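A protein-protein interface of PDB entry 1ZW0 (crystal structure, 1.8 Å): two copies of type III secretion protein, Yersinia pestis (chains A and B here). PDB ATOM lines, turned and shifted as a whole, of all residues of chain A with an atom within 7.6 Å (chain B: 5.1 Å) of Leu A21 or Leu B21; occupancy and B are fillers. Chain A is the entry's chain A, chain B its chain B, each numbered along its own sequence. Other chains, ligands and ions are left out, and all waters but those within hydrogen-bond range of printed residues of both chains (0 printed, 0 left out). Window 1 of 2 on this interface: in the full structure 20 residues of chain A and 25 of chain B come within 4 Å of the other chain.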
ATOM      1  N   THR A  13      13.145  -2.245  25.567  1.00  0.00           N
ATOM      2  CA  THR A  13      13.203  -3.729  25.433  1.00  0.00           C
ATOM      3  C   THR A  13      12.103  -4.194  24.467  1.00  0.00           C
ATOM      4  O   THR A  13      12.341  -5.064  23.611  1.00  0.00           O
ATOM      5  CB  THR A  13      13.094  -4.373  26.811  1.00  0.00           C
ATOM      6  OG1 THR A  13      14.213  -3.954  27.623  1.00  0.00           O
ATOM      7  CG2 THR A  13      13.138  -5.862  26.735  1.00  0.00           C
ATOM      8  N   VAL A  14      10.916  -3.587  24.606  1.00  0.00           N
ATOM      9  CA  VAL A  14       9.788  -3.823  23.657  1.00  0.00           C
ATOM     10  C   VAL A  14      10.236  -3.465  22.255  1.00  0.00           C
ATOM     11  O   VAL A  14      10.103  -4.269  21.339  1.00  0.00           O
ATOM     12  CB  VAL A  14       8.454  -3.124  24.096  1.00  0.00           C
ATOM     13  CG1 VAL A  14       7.481  -3.264  22.974  1.00  0.00           C
ATOM     14  CG2 VAL A  14       7.986  -3.736  25.402  1.00  0.00           C
ATOM     15  N   ARG A  15      10.828  -2.308  22.035  1.00  0.00           N
ATOM     16  CA  ARG A  15      11.318  -1.949  20.693  1.00  0.00           C
ATOM     17  C   ARG A  15      12.270  -2.985  20.124  1.00  0.00           C
ATOM     18  O   ARG A  15      12.154  -3.342  18.957  1.00  0.00           O
ATOM     19  CB  ARG A  15      12.095  -0.650  20.732  1.00  0.00           C
ATOM     20  CG  ARG A  15      12.460  -0.077  19.403  1.00  0.00           C
ATOM     21  CD  ARG A  15      13.061   1.348  19.627  1.00  0.00           C
ATOM     22  NE  ARG A  15      14.204   1.432  20.544  1.00  0.00           N
ATOM     23  CZ  ARG A  15      14.903   2.570  20.749  1.00  0.00           C
ATOM     24  NH1 ARG A  15      14.563   3.708  20.149  1.00  0.00           N
ATOM     25  NH2 ARG A  15      15.929   2.592  21.559  1.00  0.00           N
ATOM     26  N   SER A  16      13.241  -3.418  20.922  1.00  0.00           N
ATOM     27  CA  SER A  16      14.248  -4.363  20.497  1.00  0.00           C
ATOM     28  C   SER A  16      13.602  -5.657  20.086  1.00  0.00           C
ATOM     29  O   SER A  16      13.953  -6.243  19.052  1.00  0.00           O
ATOM     30  CB  SER A  16      15.229  -4.583  21.656  1.00  0.00           C
ATOM     31  OG  SER A  16      16.134  -5.610  21.378  1.00  0.00           O
ATOM     32  N   ILE A  17      12.718  -6.160  20.932  1.00  0.00           N
ATOM     33  CA  ILE A  17      12.068  -7.425  20.645  1.00  0.00           C
ATOM     34  C   ILE A  17      11.185  -7.351  19.429  1.00  0.00           C
ATOM     35  O   ILE A  17      11.168  -8.254  18.588  1.00  0.00           O
ATOM     36  CB  ILE A  17      11.391  -7.936  21.853  1.00  0.00           C
ATOM     37  CG1 ILE A  17      12.377  -8.225  22.957  1.00  0.00           C
ATOM     38  CG2 ILE A  17      10.589  -9.239  21.557  1.00  0.00           C
ATOM     39  CD1 ILE A  17      11.764  -8.583  24.322  1.00  0.00           C
ATOM     40  N   THR A  18      10.398  -6.285  19.283  1.00  0.00           N
ATOM     41  CA  THR A  18       9.578  -6.182  18.141  1.00  0.00           C
ATOM     42  C   THR A  18      10.372  -6.061  16.804  1.00  0.00           C
ATOM     43  O   THR A  18      10.016  -6.610  15.778  1.00  0.00           O
ATOM     44  CB  THR A  18       8.545  -5.057  18.301  1.00  0.00           C
ATOM     45  OG1 THR A  18       7.584  -5.289  19.356  1.00  0.00           O
ATOM     46  CG2 THR A  18       8.001  -4.483  17.044  1.00  0.00           C
ATOM     47  N   MET A  19      11.486  -5.367  16.828  1.00  0.00           N
ATOM     48  CA  MET A  19      12.406  -5.364  15.680  1.00  0.00           C
ATOM     49  C   MET A  19      12.885  -6.784  15.341  1.00  0.00           C
ATOM     50  O   MET A  19      12.898  -7.173  14.167  1.00  0.00           O
ATOM     51  CB  MET A  19      13.650  -4.508  16.003  1.00  0.00           C
ATOM     52  CG  MET A  19      14.487  -4.310  14.819  1.00  0.00           C
ATOM     53  SD  MET A  19      15.878  -3.195  15.146  1.00  0.00           S
ATOM     54  CE  MET A  19      16.943  -4.346  16.018  1.00  0.00           C
ATOM     55  N   GLN A  20      13.237  -7.547  16.360  1.00  0.00           N
ATOM     56  CA  GLN A  20      13.694  -8.947  16.145  1.00  0.00           C
ATOM     57  C   GLN A  20      12.553  -9.793  15.576  1.00  0.00           C
ATOM     58  O   GLN A  20      12.792 -10.595  14.650  1.00  0.00           O
ATOM     59  CB  GLN A  20      14.146  -9.541  17.438  1.00  0.00           C
ATOM     60  CG  GLN A  20      15.386  -8.914  18.086  1.00  0.00           C
ATOM     61  CD  GLN A  20      15.688  -9.482  19.480  1.00  0.00           C
ATOM     62  OE1 GLN A  20      15.781 -10.717  19.658  1.00  0.00           O
ATOM     63  NE2 GLN A  20      15.884  -8.604  20.477  1.00  0.00           N
ATOM     64  N   LEU A  21      11.329  -9.640  16.108  1.00  0.00           N
ATOM     65  CA  LEU A  21      10.180 -10.352  15.559  1.00  0.00           C
ATOM     66  C   LEU A  21       9.943 -10.055  14.072  1.00  0.00           C
ATOM     67  O   LEU A  21       9.720 -10.970  13.249  1.00  0.00           O
ATOM     68  CB  LEU A  21       8.890 -10.051  16.340  1.00  0.00           C
ATOM     69  CG  LEU A  21       7.613 -10.816  16.035  1.00  0.00           C
ATOM     70  CD1 LEU A  21       7.961 -12.347  15.954  1.00  0.00           C
ATOM     71  CD2 LEU A  21       6.509 -10.557  17.102  1.00  0.00           C
ATOM     72  N   GLU A  22      10.007  -8.794  13.712  1.00  0.00           N
ATOM     73  CA  GLU A  22       9.788  -8.393  12.333  1.00  0.00           C
ATOM     74  C   GLU A  22      10.828  -9.020  11.427  1.00  0.00           C
ATOM     75  O   GLU A  22      10.484  -9.550  10.369  1.00  0.00           O
ATOM     76  CB  GLU A  22       9.788  -6.855  12.207  1.00  0.00           C
ATOM     77  CG  GLU A  22       8.625  -6.145  12.858  1.00  0.00           C
ATOM     78  CD  GLU A  22       7.320  -6.188  12.101  1.00  0.00           C
ATOM     79  OE1 GLU A  22       7.141  -7.107  11.284  1.00  0.00           O
ATOM     80  OE2 GLU A  22       6.443  -5.270  12.320  1.00  0.00           O
ATOM     81  N   MET A  23      12.089  -9.036  11.856  1.00  0.00           N
ATOM     82  CA  MET A  23      13.133  -9.728  11.093  1.00  0.00           C
ATOM     83  C   MET A  23      12.876 -11.229  10.938  1.00  0.00           C
ATOM     84  O   MET A  23      13.033 -11.772   9.876  1.00  0.00           O
ATOM     85  CB  MET A  23      14.514  -9.535  11.746  1.00  0.00           C
ATOM     86  CG  MET A  23      14.991  -8.058  11.707  1.00  0.00           C
ATOM     87  SD  MET A  23      15.335  -7.584   9.990  1.00  0.00           S
ATOM     88  CE  MET A  23      13.702  -7.106   9.270  1.00  0.00           C
ATOM     89  N   ALA A  24      12.434 -11.887  12.003  1.00  0.00           N
ATOM     90  CA  ALA A  24      12.146 -13.307  11.938  1.00  0.00           C
ATOM     91  C   ALA A  24      10.928 -13.623  11.035  1.00  0.00           C
ATOM     92  O   ALA A  24      10.846 -14.661  10.342  1.00  0.00           O
ATOM     93  CB  ALA A  24      11.869 -13.823  13.383  1.00  0.00           C
ATOM     94  N   LEU A  25       9.951 -12.743  11.068  1.00  0.00           N
ATOM     95  CA  LEU A  25       8.801 -12.874  10.158  1.00  0.00           C
ATOM     96  C   LEU A  25       9.242 -12.699   8.690  1.00  0.00           C
ATOM     97  O   LEU A  25       8.775 -13.392   7.819  1.00  0.00           O
ATOM     98  CB  LEU A  25       7.712 -11.858  10.506  1.00  0.00           C
ATOM     99  CG  LEU A  25       6.949 -12.240  11.770  1.00  0.00           C
ATOM    100  CD1 LEU A  25       6.053 -11.104  12.229  1.00  0.00           C
ATOM    101  CD2 LEU A  25       6.060 -13.414  11.512  1.00  0.00           C
ATOM    102  N   THR A  26      10.159 -11.783   8.435  1.00  0.00           N
ATOM    103  CA  THR A  26      10.697 -11.678   7.071  1.00  0.00           C
ATOM    104  C   THR A  26      11.346 -12.978   6.550  1.00  0.00           C
ATOM    105  O   THR A  26      11.192 -13.350   5.373  1.00  0.00           O
ATOM    106  CB  THR A  26      11.709 -10.503   7.003  1.00  0.00           C
ATOM    107  OG1 THR A  26      11.005  -9.305   7.320  1.00  0.00           O
ATOM    108  CG2 THR A  26      12.272 -10.389   5.625  1.00  0.00           C
ATOM    109  N   LYS A  27      12.079 -13.674   7.412  1.00  0.00           N
ATOM    110  CA  LYS A  27      12.740 -14.926   7.036  1.00  0.00           C
ATOM    111  C   LYS A  27      11.741 -16.047   6.806  1.00  0.00           C
ATOM    112  O   LYS A  27      11.827 -16.791   5.805  1.00  0.00           O
ATOM    113  CB  LYS A  27      13.712 -15.342   8.107  1.00  0.00           C
ATOM    114  CG  LYS A  27      14.948 -14.532   8.111  1.00  0.00           C
ATOM    115  CD  LYS A  27      15.991 -15.017   9.172  1.00  0.00           C
ATOM    116  CE  LYS A  27      16.176 -16.559   9.282  1.00  0.00           C
ATOM    117  NZ  LYS A  27      16.823 -17.292   8.118  1.00  0.00           N
ATOM    118  N   LEU A  28      10.749 -16.141   7.707  1.00  0.00           N
ATOM    119  CA  LEU A  28       9.702 -17.140   7.621  1.00  0.00           C
ATOM    120  C   LEU A  28       8.977 -16.915   6.328  1.00  0.00           C
ATOM    121  O   LEU A  28       8.620 -17.860   5.613  1.00  0.00           O
ATOM    122  CB  LEU A  28       8.745 -17.035   8.809  1.00  0.00           C
ATOM    123  CG  LEU A  28       7.606 -18.042   8.864  1.00  0.00           C
ATOM    124  CD1 LEU A  28       8.070 -19.390   8.569  1.00  0.00           C
ATOM    125  CD2 LEU A  28       6.956 -18.017  10.252  1.00  0.00           C
ATOM    126  N   LEU A  51      -0.288 -11.275  12.648  1.00  0.00           N
ATOM    127  CA  LEU A  51       0.834 -11.032  13.506  1.00  0.00           C
ATOM    128  C   LEU A  51       1.362  -9.629  13.316  1.00  0.00           C
ATOM    129  O   LEU A  51       1.697  -8.943  14.272  1.00  0.00           O
ATOM    130  CB  LEU A  51       1.976 -12.001  13.145  1.00  0.00           C
ATOM    131  CG  LEU A  51       1.805 -13.273  13.874  1.00  0.00           C
ATOM    132  CD1 LEU A  51       2.589 -14.416  13.213  1.00  0.00           C
ATOM    133  CD2 LEU A  51       2.206 -13.061  15.333  1.00  0.00           C
ATOM    134  N   GLU A  52       1.452  -9.213  12.053  1.00  0.00           N
ATOM    135  CA  GLU A  52       1.977  -7.895  11.810  1.00  0.00           C
ATOM    136  C   GLU A  52       0.954  -6.863  12.368  1.00  0.00           C
ATOM    137  O   GLU A  52       1.357  -5.863  12.858  1.00  0.00           O
ATOM    138  CB  GLU A  52       2.153  -7.666  10.334  1.00  0.00           C
ATOM    139  CG  GLU A  52       3.130  -8.606   9.646  1.00  0.00           C
ATOM    140  CD  GLU A  52       4.565  -8.299   9.916  1.00  0.00           C
ATOM    141  OE1 GLU A  52       4.915  -7.452  10.796  1.00  0.00           O
ATOM    142  OE2 GLU A  52       5.389  -8.985   9.267  1.00  0.00           O
ATOM    143  N   ALA A  54      -0.895  -7.310  14.970  1.00  0.00           N
ATOM    144  CA  ALA A  54      -0.671  -7.273  16.441  1.00  0.00           C
ATOM    145  C   ALA A  54       0.536  -6.479  16.800  1.00  0.00           C
ATOM    146  O   ALA A  54       0.600  -5.701  17.763  1.00  0.00           O
ATOM    147  CB  ALA A  54      -0.664  -8.681  17.009  1.00  0.00           C
ATOM    148  N   ILE A  55       1.577  -6.574  15.992  1.00  0.00           N
ATOM    149  CA  ILE A  55       2.695  -5.732  16.238  1.00  0.00           C
ATOM    150  C   ILE A  55       2.398  -4.249  16.086  1.00  0.00           C
ATOM    151  O   ILE A  55       2.851  -3.440  16.907  1.00  0.00           O
ATOM    152  CB  ILE A  55       3.923  -6.171  15.322  1.00  0.00           C
ATOM    153  CG1 ILE A  55       4.389  -7.606  15.727  1.00  0.00           C
ATOM    154  CG2 ILE A  55       4.998  -5.105  15.334  1.00  0.00           C
ATOM    155  CD1 ILE A  55       5.317  -8.097  14.621  1.00  0.00           C
ATOM    156  N   ILE A  58       0.778  -3.053  19.194  1.00  0.00           N
ATOM    157  CA  ILE A  58       1.772  -2.904  20.231  1.00  0.00           C
ATOM    158  C   ILE A  58       2.495  -1.598  20.096  1.00  0.00           C
ATOM    159  O   ILE A  58       2.674  -0.890  21.054  1.00  0.00           O
ATOM    160  CB  ILE A  58       2.715  -4.141  20.238  1.00  0.00           C
ATOM    161  CG1 ILE A  58       1.929  -5.316  20.743  1.00  0.00           C
ATOM    162  CG2 ILE A  58       3.895  -3.812  21.075  1.00  0.00           C
ATOM    163  CD1 ILE A  58       2.596  -6.656  20.590  1.00  0.00           C
ATOM    164  N   ASP A  64       6.764   2.432  21.186  1.00  0.00           N
ATOM    165  CA  ASP A  64       8.225   2.219  21.093  1.00  0.00           C
ATOM    166  C   ASP A  64       8.824   2.801  19.815  1.00  0.00           C
ATOM    167  O   ASP A  64      10.027   3.083  19.773  1.00  0.00           O
ATOM    168  CB  ASP A  64       8.529   0.747  21.159  1.00  0.00           C
ATOM    169  CG  ASP A  64       7.844  -0.041  20.080  1.00  0.00           C
ATOM    170  OD1 ASP A  64       6.614   0.101  19.857  1.00  0.00           O
ATOM    171  OD2 ASP A  64       8.536  -0.857  19.467  1.00  0.00           O
ATOM    172  N   VAL B  14      10.163 -17.369  15.409  1.00  0.00           N
ATOM    173  CA  VAL B  14       8.982 -16.489  15.468  1.00  0.00           C
ATOM    174  C   VAL B  14       8.223 -16.818  16.750  1.00  0.00           C
ATOM    175  O   VAL B  14       7.843 -15.925  17.483  1.00  0.00           O
ATOM    176  CB  VAL B  14       8.075 -16.640  14.261  1.00  0.00           C
ATOM    177  CG1 VAL B  14       6.753 -15.840  14.455  1.00  0.00           C
ATOM    178  CG2 VAL B  14       8.854 -16.070  13.049  1.00  0.00           C
ATOM    179  N   ILE B  17      10.251 -15.599  19.845  1.00  0.00           N
ATOM    180  CA  ILE B  17      10.296 -14.123  19.993  1.00  0.00           C
ATOM    181  C   ILE B  17       8.897 -13.597  20.402  1.00  0.00           C
ATOM    182  O   ILE B  17       8.810 -12.631  21.195  1.00  0.00           O
ATOM    183  CB  ILE B  17      10.880 -13.402  18.750  1.00  0.00           C
ATOM    184  CG1 ILE B  17      12.316 -13.852  18.472  1.00  0.00           C
ATOM    185  CG2 ILE B  17      10.940 -11.871  18.940  1.00  0.00           C
ATOM    186  CD1 ILE B  17      12.786 -13.481  17.099  1.00  0.00           C
ATOM    187  N   THR B  18       7.821 -14.182  19.900  1.00  0.00           N
ATOM    188  CA  THR B  18       6.498 -13.727  20.314  1.00  0.00           C
ATOM    189  C   THR B  18       6.274 -13.956  21.817  1.00  0.00           C
ATOM    190  O   THR B  18       5.781 -13.046  22.513  1.00  0.00           O
ATOM    191  CB  THR B  18       5.426 -14.368  19.499  1.00  0.00           C
ATOM    192  OG1 THR B  18       5.640 -14.034  18.106  1.00  0.00           O
ATOM    193  CG2 THR B  18       4.130 -13.867  19.910  1.00  0.00           C
ATOM    194  N   MET B  19       6.742 -15.085  22.353  1.00  0.00           N
ATOM    195  CA  MET B  19       6.628 -15.328  23.808  1.00  0.00           C
ATOM    196  C   MET B  19       7.483 -14.291  24.601  1.00  0.00           C
ATOM    197  O   MET B  19       7.055 -13.838  25.654  1.00  0.00           O
ATOM    198  CB  MET B  19       6.954 -16.777  24.177  1.00  0.00           C
ATOM    199  CG  MET B  19       5.896 -17.774  23.626  1.00  0.00           C
ATOM    200  SD  MET B  19       6.128 -19.546  23.988  1.00  0.00           S
ATOM    201  CE  MET B  19       7.702 -19.948  23.293  1.00  0.00           C
ATOM    202  N   GLN B  20       8.676 -13.936  24.085  1.00  0.00           N
ATOM    203  CA  GLN B  20       9.528 -12.931  24.679  1.00  0.00           C
ATOM    204  C   GLN B  20       8.857 -11.590  24.690  1.00  0.00           C
ATOM    205  O   GLN B  20       8.944 -10.849  25.639  1.00  0.00           O
ATOM    206  CB  GLN B  20      10.826 -12.807  23.946  1.00  0.00           C
ATOM    207  CG  GLN B  20      11.666 -14.100  24.063  1.00  0.00           C
ATOM    208  CD  GLN B  20      12.930 -13.998  23.263  1.00  0.00           C
ATOM    209  OE1 GLN B  20      13.721 -13.150  23.573  1.00  0.00           O
ATOM    210  NE2 GLN B  20      13.166 -14.926  22.282  1.00  0.00           N
ATOM    211  N   LEU B  21       8.179 -11.269  23.610  1.00  0.00           N
ATOM    212  CA  LEU B  21       7.481  -9.989  23.521  1.00  0.00           C
ATOM    213  C   LEU B  21       6.344  -9.932  24.568  1.00  0.00           C
ATOM    214  O   LEU B  21       6.073  -8.871  25.189  1.00  0.00           O
ATOM    215  CB  LEU B  21       7.009  -9.825  22.079  1.00  0.00           C
ATOM    216  CG  LEU B  21       6.266  -8.524  21.752  1.00  0.00           C
ATOM    217  CD1 LEU B  21       7.101  -7.334  22.194  1.00  0.00           C
ATOM    218  CD2 LEU B  21       5.903  -8.475  20.309  1.00  0.00           C
ATOM    219  N   GLU B  22       5.630 -11.043  24.715  1.00  0.00           N
ATOM    220  CA  GLU B  22       4.573 -11.188  25.716  1.00  0.00           C
ATOM    221  C   GLU B  22       5.160 -10.870  27.084  1.00  0.00           C
ATOM    222  O   GLU B  22       4.606 -10.079  27.834  1.00  0.00           O
ATOM    223  CB  GLU B  22       3.953 -12.514  25.664  1.00  0.00           C
ATOM    224  CG  GLU B  22       3.103 -12.793  24.441  1.00  0.00           C
ATOM    225  CD  GLU B  22       2.544 -14.175  24.431  1.00  0.00           C
ATOM    226  OE1 GLU B  22       1.997 -14.613  25.462  1.00  0.00           O
ATOM    227  OE2 GLU B  22       2.671 -14.876  23.393  1.00  0.00           O
ATOM    228  N   MET B  23       6.303 -11.451  27.424  1.00  0.00           N
ATOM    229  CA  MET B  23       6.920 -11.153  28.705  1.00  0.00           C
ATOM    230  C   MET B  23       7.383  -9.700  28.840  1.00  0.00           C
ATOM    231  O   MET B  23       7.295  -9.113  29.937  1.00  0.00           O
ATOM    232  CB  MET B  23       8.099 -12.084  28.951  1.00  0.00           C
ATOM    233  CG  MET B  23       7.704 -13.518  29.125  1.00  0.00           C
ATOM    234  SD  MET B  23       9.019 -14.647  29.557  1.00  0.00           S
ATOM    235  CE  MET B  23       9.370 -14.207  31.270  1.00  0.00           C
ATOM    236  N   ALA B  24       7.877  -9.084  27.777  1.00  0.00           N
ATOM    237  CA  ALA B  24       8.396  -7.705  27.833  1.00  0.00           C
ATOM    238  C   ALA B  24       7.253  -6.765  28.086  1.00  0.00           C
ATOM    239  O   ALA B  24       7.365  -5.772  28.799  1.00  0.00           O
ATOM    240  CB  ALA B  24       9.088  -7.334  26.527  1.00  0.00           C
ATOM    241  N   LEU B  25       6.130  -7.021  27.404  1.00  0.00           N
ATOM    242  CA  LEU B  25       4.930  -6.176  27.598  1.00  0.00           C
ATOM    243  C   LEU B  25       4.362  -6.369  29.000  1.00  0.00           C
ATOM    244  O   LEU B  25       3.810  -5.428  29.621  1.00  0.00           O
ATOM    245  CB  LEU B  25       3.887  -6.585  26.578  1.00  0.00           C
ATOM    246  CG  LEU B  25       4.240  -6.243  25.118  1.00  0.00           C
ATOM    247  CD1 LEU B  25       3.259  -7.003  24.181  1.00  0.00           C
ATOM    248  CD2 LEU B  25       4.235  -4.755  24.775  1.00  0.00           C
ATOM    249  N   THR B  26       4.462  -7.580  29.497  1.00  0.00           N
ATOM    250  CA  THR B  26       3.985  -7.904  30.873  1.00  0.00           C
ATOM    251  C   THR B  26       4.810  -7.078  31.892  1.00  0.00           C
ATOM    252  O   THR B  26       4.260  -6.531  32.855  1.00  0.00           O
ATOM    253  CB  THR B  26       4.063  -9.385  31.198  1.00  0.00           C
ATOM    254  OG1 THR B  26       3.138 -10.081  30.344  1.00  0.00           O
ATOM    255  CG2 THR B  26       3.711  -9.663  32.647  1.00  0.00           C
ATOM    256  N   ILE B  58      -1.589 -11.291  20.677  1.00  0.00           N
ATOM    257  CA  ILE B  58      -0.464 -11.898  20.037  1.00  0.00           C
ATOM    258  C   ILE B  58      -0.253 -13.360  20.493  1.00  0.00           C
ATOM    259  O   ILE B  58       0.081 -14.246  19.675  1.00  0.00           O
ATOM    260  CB  ILE B  58       0.784 -10.942  20.161  1.00  0.00           C
ATOM    261  CG1 ILE B  58       1.613 -11.155  18.865  1.00  0.00           C
ATOM    262  CG2 ILE B  58       1.329 -11.158  21.515  1.00  0.00           C
ATOM    263  CD1 ILE B  58       2.917 -10.474  18.790  1.00  0.00           C
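Printed residues of chain B within 4 Å of Val A14: Ala B24 (3.9 Å) and Leu B25 (3.9 Å). Printed residues of chain B within 4 Å of Thr A18: Leu B21 (3.5 Å). Of chain B, only Val B14 (3.9 Å), Ile B17 (3.6 Å), Thr B18 (3.6 Å), Leu B21 (3.9 Å) and Ile B58 (3.97 Å) come within 4 Å of Leu A21. Printed residues of chain A within 4 Å of Thr B18: Leu A21. Printed residues of chain A within 4 Å of Leu B21: Ile A17, Thr A18, Leu A21 and Ile A58. Printed residues of chain A within 4 Å of Leu B25: Val A14 and Ile A58. The nearest printed residue of chain A that does not touch Leu B21 is Val A14 (4.2 Å).
O of Val A14 is in hydrogen-bond range of OG1 of Thr A18 (3.4 Å). OG of Ser A16 sits at hydrogen-bond distance from NE2 of Gln A20, 3.1 Å away. The backbone carbonyl oxygen of Val B14 lies within hydrogen-bond range of the side-chain hydroxyl of Thr B18 (3.0 Å).
Val A14 touches Ala B24, and with the chains exchanged Ala A24 touches Val B14. Val A14 touches Leu B25, and with the chains exchanged Leu A25 touches Val B14. Ile B17 touches its own counterpart, Ile A17. Leu B21 touches its own counterpart, Leu A21. Positions printed for both chains: 14, 17, 18, 19, 20, 21, 22, 23, 24, 25, 26 and 58.
Of the 12 printed residues of chain B, 8 touch a printed residue of chain A. Printed residues of chain B that touch a printed residue of chain A: Val B14, Ile B17, Thr B18, Gln B20, Leu B21, Ala B24, Leu B25 and Ile B58. Among the printed residues, no Asp or Glu carboxylate lies within 4 Å of a Lys or Arg side-chain nitrogen of the other chain.
Val A14 touches Ala B24. Leu B25 touches Val A14 (CD2 to CG2, 3.9 Å). Ile A17 touches Leu B21 (CG2 to CB, 3.7 Å). Ile A17 touches Ala B24 (CD1 to CB, 3.7 Å). Thr A18 touches Leu B21. CD1 of Leu A21 touches OG1 of Thr B18, 3.6 Å away. CD2 of Leu A21 touches CD1 of Ile B58, at 3.97 Å. O of Ala A24 touches CG2 of Val B14, 3.6 Å away. Ile B58 touches Ala A54. Leu B25 touches Ile A58.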
